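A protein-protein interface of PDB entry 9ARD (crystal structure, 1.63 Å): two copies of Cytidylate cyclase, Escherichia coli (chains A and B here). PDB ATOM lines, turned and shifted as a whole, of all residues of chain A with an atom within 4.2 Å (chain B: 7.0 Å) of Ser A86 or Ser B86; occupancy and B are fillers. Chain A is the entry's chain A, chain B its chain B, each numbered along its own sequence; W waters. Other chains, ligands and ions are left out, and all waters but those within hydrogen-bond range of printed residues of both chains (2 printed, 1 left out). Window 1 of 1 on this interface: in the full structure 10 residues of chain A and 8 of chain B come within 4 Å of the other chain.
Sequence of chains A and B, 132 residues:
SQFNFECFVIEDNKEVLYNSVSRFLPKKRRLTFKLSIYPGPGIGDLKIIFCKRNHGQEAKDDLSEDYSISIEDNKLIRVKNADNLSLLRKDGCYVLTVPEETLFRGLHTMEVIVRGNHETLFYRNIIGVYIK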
ATOM      1  N   ARG A  78      26.739  -7.848  20.316  1.00  0.00           N
ATOM      2  CA  ARG A  78      26.618  -6.425  20.623  1.00  0.00           C
ATOM      3  C   ARG A  78      26.477  -6.251  22.128  1.00  0.00           C
ATOM      4  O   ARG A  78      25.474  -6.672  22.715  1.00  0.00           O
ATOM      5  CB  ARG A  78      25.419  -5.817  19.903  1.00  0.00           C
ATOM      6  CG  ARG A  78      25.746  -5.170  18.580  1.00  0.00           C
ATOM      7  CD  ARG A  78      25.571  -6.131  17.427  1.00  0.00           C
ATOM      8  NE  ARG A  78      25.764  -5.454  16.151  1.00  0.00           N
ATOM      9  CZ  ARG A  78      25.630  -6.034  14.968  1.00  0.00           C
ATOM     10  NH1 ARG A  78      25.276  -7.303  14.857  1.00  0.00           N
ATOM     11  NH2 ARG A  78      25.864  -5.324  13.869  1.00  0.00           N
ATOM     12  N   ASN A  84      25.709   0.310  15.200  1.00  0.00           N
ATOM     13  CA  ASN A  84      26.228   0.685  13.894  1.00  0.00           C
ATOM     14  C   ASN A  84      27.414  -0.163  13.458  1.00  0.00           C
ATOM     15  O   ASN A  84      27.843  -0.052  12.305  1.00  0.00           O
ATOM     16  CB  ASN A  84      26.614   2.170  13.891  1.00  0.00           C
ATOM     17  CG  ASN A  84      25.426   3.076  14.162  1.00  0.00           C
ATOM     18  OD1 ASN A  84      24.281   2.722  13.872  1.00  0.00           O
ATOM     19  ND2 ASN A  84      25.691   4.253  14.718  1.00  0.00           N
ATOM     20  N   LEU A  85      27.948  -1.006  14.336  1.00  0.00           N
ATOM     21  CA  LEU A  85      29.066  -1.852  13.964  1.00  0.00           C
ATOM     22  C   LEU A  85      28.577  -3.046  13.148  1.00  0.00           C
ATOM     23  O   LEU A  85      27.405  -3.429  13.195  1.00  0.00           O
ATOM     24  CB  LEU A  85      29.825  -2.323  15.206  1.00  0.00           C
ATOM     25  CG  LEU A  85      30.842  -1.349  15.810  1.00  0.00           C
ATOM     26  CD1 LEU A  85      30.194  -0.054  16.284  1.00  0.00           C
ATOM     27  CD2 LEU A  85      31.609  -2.012  16.950  1.00  0.00           C
ATOM     28  N   SER A  86      29.493  -3.622  12.371  1.00  0.00           N
ATOM     29  CA  SER A  86      29.178  -4.782  11.550  1.00  0.00           C
ATOM     30  C   SER A  86      30.432  -5.630  11.399  1.00  0.00           C
ATOM     31  O   SER A  86      31.553  -5.114  11.401  1.00  0.00           O
ATOM     32  CB  SER A  86      28.631  -4.374  10.175  1.00  0.00           C
ATOM     33  OG  SER A  86      29.606  -3.683   9.414  1.00  0.00           O
ATOM     34  N   LEU A  87      30.230  -6.940  11.275  1.00  0.00           N
ATOM     35  CA  LEU A  87      31.316  -7.907  11.179  1.00  0.00           C
ATOM     36  C   LEU A  87      31.208  -8.649   9.855  1.00  0.00           C
ATOM     37  O   LEU A  87      30.121  -9.100   9.482  1.00  0.00           O
ATOM     38  CB  LEU A  87      31.274  -8.893  12.353  1.00  0.00           C
ATOM     39  CG  LEU A  87      32.406  -9.915  12.507  1.00  0.00           C
ATOM     40  CD1 LEU A  87      33.760  -9.232  12.604  1.00  0.00           C
ATOM     41  CD2 LEU A  87      32.169 -10.793  13.731  1.00  0.00           C
ATOM     42  N   VAL A  95      36.600  -8.712   9.722  1.00  0.00           N
ATOM     43  CA  VAL A  95      36.696  -7.260   9.620  1.00  0.00           C
ATOM     44  C   VAL A  95      35.511  -6.656  10.354  1.00  0.00           C
ATOM     45  O   VAL A  95      34.352  -6.939  10.016  1.00  0.00           O
ATOM     46  CB  VAL A  95      36.727  -6.785   8.159  1.00  0.00           C
ATOM     47  CG1 VAL A  95      36.949  -5.278   8.107  1.00  0.00           C
ATOM     48  CG2 VAL A  95      37.807  -7.514   7.386  1.00  0.00           C
ATOM     49  N   LEU A  96      35.807  -5.827  11.347  1.00  0.00           N
ATOM     50  CA  LEU A  96      34.818  -5.081  12.107  1.00  0.00           C
ATOM     51  C   LEU A  96      34.874  -3.628  11.657  1.00  0.00           C
ATOM     52  O   LEU A  96      35.941  -3.010  11.689  1.00  0.00           O
ATOM     53  CB  LEU A  96      35.100  -5.197  13.605  1.00  0.00           C
ATOM     54  CG  LEU A  96      34.007  -4.794  14.591  1.00  0.00           C
ATOM     55  CD1 LEU A  96      32.726  -5.536  14.285  1.00  0.00           C
ATOM     56  CD2 LEU A  96      34.470  -5.107  16.000  1.00  0.00           C
ATOM     57  N   THR A  97      33.733  -3.091  11.238  1.00  0.00           N
ATOM     58  CA  THR A  97      33.671  -1.752  10.665  1.00  0.00           C
ATOM     59  C   THR A  97      32.860  -0.835  11.565  1.00  0.00           C
ATOM     60  O   THR A  97      31.765  -1.202  12.007  1.00  0.00           O
ATOM     61  CB  THR A  97      33.067  -1.796   9.262  1.00  0.00           C
ATOM     62  OG1 THR A  97      33.903  -2.593   8.415  1.00  0.00           O
ATOM     63  CG2 THR A  97      32.947  -0.393   8.677  1.00  0.00           C
ATOM     64  N   LEU B  76      16.953  -0.593  14.100  1.00  0.00           N
ATOM     65  CA  LEU B  76      17.039  -1.890  13.442  1.00  0.00           C
ATOM     66  C   LEU B  76      16.791  -3.005  14.447  1.00  0.00           C
ATOM     67  O   LEU B  76      17.399  -3.035  15.523  1.00  0.00           O
ATOM     68  CB  LEU B  76      18.406  -2.083  12.786  1.00  0.00           C
ATOM     69  CG  LEU B  76      18.585  -3.441  12.092  1.00  0.00           C
ATOM     70  CD1 LEU B  76      17.645  -3.558  10.905  1.00  0.00           C
ATOM     71  CD2 LEU B  76      20.025  -3.686  11.658  1.00  0.00           C
ATOM     72  N   ARG B  78      16.930  -7.122  14.484  1.00  0.00           N
ATOM     73  CA  ARG B  78      17.351  -8.318  13.766  1.00  0.00           C
ATOM     74  C   ARG B  78      16.421  -9.458  14.159  1.00  0.00           C
ATOM     75  O   ARG B  78      16.475  -9.952  15.289  1.00  0.00           O
ATOM     76  CB  ARG B  78      18.809  -8.632  14.084  1.00  0.00           C
ATOM     77  CG  ARG B  78      19.724  -7.478  13.725  1.00  0.00           C
ATOM     78  CD  ARG B  78      21.060  -7.533  14.443  1.00  0.00           C
ATOM     79  NE  ARG B  78      21.911  -6.436  14.003  1.00  0.00           N
ATOM     80  CZ  ARG B  78      22.561  -6.425  12.847  1.00  0.00           C
ATOM     81  NH1 ARG B  78      22.529  -7.464  12.027  1.00  0.00           N
ATOM     82  NH2 ARG B  78      23.253  -5.346  12.502  1.00  0.00           N
ATOM     83  N   ALA B  82      19.911 -12.663  10.672  1.00  0.00           N
ATOM     84  CA  ALA B  82      20.231 -11.332  10.170  1.00  0.00           C
ATOM     85  C   ALA B  82      21.504 -10.765  10.784  1.00  0.00           C
ATOM     86  O   ALA B  82      21.676  -9.544  10.818  1.00  0.00           O
ATOM     87  CB  ALA B  82      19.062 -10.377  10.420  1.00  0.00           C
ATOM     88  N   ASP B  83      22.404 -11.626  11.265  1.00  0.00           N
ATOM     89  CA  ASP B  83      23.601 -11.134  11.941  1.00  0.00           C
ATOM     90  C   ASP B  83      24.556 -10.427  10.984  1.00  0.00           C
ATOM     91  O   ASP B  83      25.289  -9.524  11.404  1.00  0.00           O
ATOM     92  CB  ASP B  83      24.310 -12.283  12.653  1.00  0.00           C
ATOM     93  CG  ASP B  83      23.557 -12.760  13.882  1.00  0.00           C
ATOM     94  OD1 ASP B  83      22.749 -11.976  14.425  1.00  0.00           O
ATOM     95  OD2 ASP B  83      23.778 -13.913  14.307  1.00  0.00           O
ATOM     96  N   ASN B  84      24.567 -10.809   9.704  1.00  0.00           N
ATOM     97  CA  ASN B  84      25.482 -10.188   8.751  1.00  0.00           C
ATOM     98  C   ASN B  84      24.949  -8.886   8.166  1.00  0.00           C
ATOM     99  O   ASN B  84      25.694  -8.190   7.463  1.00  0.00           O
ATOM    100  CB  ASN B  84      25.807 -11.158   7.611  1.00  0.00           C
ATOM    101  CG  ASN B  84      26.610 -12.358   8.075  1.00  0.00           C
ATOM    102  OD1 ASN B  84      27.340 -12.288   9.063  1.00  0.00           O
ATOM    103  ND2 ASN B  84      26.481 -13.468   7.357  1.00  0.00           N
ATOM    104  N   LEU B  85      23.698  -8.537   8.435  1.00  0.00           N
ATOM    105  CA  LEU B  85      23.124  -7.315   7.893  1.00  0.00           C
ATOM    106  C   LEU B  85      23.559  -6.104   8.708  1.00  0.00           C
ATOM    107  O   LEU B  85      23.821  -6.199   9.909  1.00  0.00           O
ATOM    108  CB  LEU B  85      21.598  -7.408   7.862  1.00  0.00           C
ATOM    109  CG  LEU B  85      20.977  -8.017   6.601  1.00  0.00           C
ATOM    110  CD1 LEU B  85      21.346  -9.485   6.434  1.00  0.00           C
ATOM    111  CD2 LEU B  85      19.468  -7.837   6.615  1.00  0.00           C
ATOM    112  N   SER B  86      23.646  -4.955   8.038  1.00  0.00           N
ATOM    113  CA  SER B  86      24.025  -3.713   8.698  1.00  0.00           C
ATOM    114  C   SER B  86      23.201  -2.570   8.126  1.00  0.00           C
ATOM    115  O   SER B  86      22.749  -2.626   6.979  1.00  0.00           O
ATOM    116  CB  SER B  86      25.527  -3.423   8.549  1.00  0.00           C
ATOM    117  OG  SER B  86      25.863  -3.059   7.221  1.00  0.00           O
ATOM    118  N   LEU B  87      23.007  -1.529   8.938  1.00  0.00           N
ATOM    119  CA  LEU B  87      22.153  -0.398   8.577  1.00  0.00           C
ATOM    120  C   LEU B  87      22.921   0.903   8.771  1.00  0.00           C
ATOM    121  O   LEU B  87      23.268   1.265   9.902  1.00  0.00           O
ATOM    122  CB  LEU B  87      20.864  -0.403   9.402  1.00  0.00           C
ATOM    123  CG  LEU B  87      19.912   0.789   9.259  1.00  0.00           C
ATOM    124  CD1 LEU B  87      19.581   1.066   7.805  1.00  0.00           C
ATOM    125  CD2 LEU B  87      18.639   0.555  10.059  1.00  0.00           C
ATOM    126  N   LEU B  88      23.177   1.611   7.671  1.00  0.00           N
ATOM    127  CA  LEU B  88      23.882   2.888   7.685  1.00  0.00           C
ATOM    128  C   LEU B  88      22.900   4.019   7.413  1.00  0.00           C
ATOM    129  O   LEU B  88      22.120   3.954   6.456  1.00  0.00           O
ATOM    130  CB  LEU B  88      25.005   2.910   6.642  1.00  0.00           C
ATOM    131  CG  LEU B  88      25.597   4.285   6.312  1.00  0.00           C
ATOM    132  CD1 LEU B  88      26.458   4.807   7.457  1.00  0.00           C
ATOM    133  CD2 LEU B  88      26.386   4.253   5.009  1.00  0.00           C
ATOM    134  N   VAL B  95      20.207   2.776   4.637  1.00  0.00           N
ATOM    135  CA  VAL B  95      20.753   1.768   3.730  1.00  0.00           C
ATOM    136  C   VAL B  95      20.976   0.478   4.507  1.00  0.00           C
ATOM    137  O   VAL B  95      21.747   0.461   5.475  1.00  0.00           O
ATOM    138  CB  VAL B  95      22.067   2.220   3.071  1.00  0.00           C
ATOM    139  CG1 VAL B  95      22.486   1.213   2.002  1.00  0.00           C
ATOM    140  CG2 VAL B  95      21.925   3.617   2.481  1.00  0.00           C
ATOM    141  N   LEU B  96      20.314  -0.600   4.074  1.00  0.00           N
ATOM    142  CA  LEU B  96      20.506  -1.939   4.619  1.00  0.00           C
ATOM    143  C   LEU B  96      21.373  -2.740   3.658  1.00  0.00           C
ATOM    144  O   LEU B  96      21.010  -2.909   2.487  1.00  0.00           O
ATOM    145  CB  LEU B  96      19.167  -2.650   4.819  1.00  0.00           C
ATOM    146  CG  LEU B  96      18.160  -2.071   5.807  1.00  0.00           C
ATOM    147  CD1 LEU B  96      16.812  -2.716   5.577  1.00  0.00           C
ATOM    148  CD2 LEU B  96      18.620  -2.315   7.233  1.00  0.00           C
ATOM    149  N   THR B  97      22.493  -3.259   4.149  1.00  0.00           N
ATOM    150  CA  THR B  97      23.457  -3.952   3.304  1.00  0.00           C
ATOM    151  C   THR B  97      23.494  -5.433   3.658  1.00  0.00           C
ATOM    152  O   THR B  97      23.651  -5.791   4.832  1.00  0.00           O
ATOM    153  CB  THR B  97      24.851  -3.339   3.449  1.00  0.00           C
ATOM    154  OG1 THR B  97      24.807  -1.952   3.077  1.00  0.00           O
ATOM    155  CG2 THR B  97      25.848  -4.066   2.561  1.00  0.00           C
ATOM    156  N   VAL B  98      23.354  -6.283   2.645  1.00  0.00           N
ATOM    157  CA  VAL B  98      23.424  -7.733   2.780  1.00  0.00           C
ATOM    158  C   VAL B  98      24.657  -8.217   2.023  1.00  0.00           C
ATOM    159  O   VAL B  98      24.695  -8.133   0.785  1.00  0.00           O
ATOM    160  CB  VAL B  98      22.151  -8.411   2.255  1.00  0.00           C
ATOM    161  CG1 VAL B  98      22.233  -9.926   2.453  1.00  0.00           C
ATOM    162  CG2 VAL B  98      20.914  -7.832   2.928  1.00  0.00           C
ATOM    163  N   PRO B  99      25.680  -8.737   2.703  1.00  0.00           N
ATOM    164  CA  PRO B  99      26.887  -9.199   2.011  1.00  0.00           C
ATOM    165  C   PRO B  99      26.781 -10.654   1.587  1.00  0.00           C
ATOM    166  O   PRO B  99      26.224 -11.499   2.291  1.00  0.00           O
ATOM    167  CB  PRO B  99      27.974  -9.023   3.080  1.00  0.00           C
ATOM    168  CG  PRO B  99      27.249  -9.323   4.353  1.00  0.00           C
ATOM    169  CD  PRO B  99      25.817  -8.846   4.168  1.00  0.00           C
HETATM  170  O   HOH W   1      22.993  -3.606  14.455  1.00  0.00           O
HETATM  171  O   HOH W   2      25.146  -2.000  11.569  1.00  0.00           O
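Of the 14 printed residues of chain B, 2 touch a printed residue of chain A.
Printed residues of chain B within 4 Å of Arg A78: Arg B78. Printed residues of chain A within 4 Å of Arg B78: Arg A78. Ser B86 touches just one residue of chain A: Ser A86. The nearest printed residue of chain A that does not touch Ser B86 is Leu A85 (5.0 Å).
O of Ser A86 sits at hydrogen-bond distance from N of Thr A97, at 3.0 Å. O of Ser B86 lies within hydrogen-bond range of N of Thr B97 (2.9 Å). NH1 of Arg B78 sits at hydrogen-bond distance from O of Ala B82. NH2 of Arg A78 sits at hydrogen-bond distance from O of Leu A85, at 2.5 Å. The backbone carbonyl oxygen (O) of Asp B83 is in hydrogen-bond range of the guanidinium group (NH1) of Arg B78 (3.5 Å). The backbone carbonyl oxygen (O) of Leu B85 lies within hydrogen-bond range of the guanidinium group (NH1) of Arg B78 (2.8 Å).
Among the printed residues, merely in contact across the chains: Ser A86 with Ser B86.
Water W1 lies within hydrogen-bond range of NH2 of Arg B78 (2.6 Å) and NH2 of Arg A78 (3.4 Å). Water W2 lies within hydrogen-bond range of the backbone carbonyl oxygen of Leu A85 (3.1 Å), the backbone carbonyl oxygen of Asn A84 (3.4 Å) and the backbone NH of Leu B87 (3.4 Å).
Arg B78 touches its own counterpart, Arg A78. Ser A86 touches its own counterpart, Ser B86. Positions printed for both chains: 78, 84, 85, 86, 87, 95, 96 and 97.
The guanidinium group (NH2) of Arg A78 sits close to the guanidinium group (NH2) of Arg B78 (2.9 Å).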
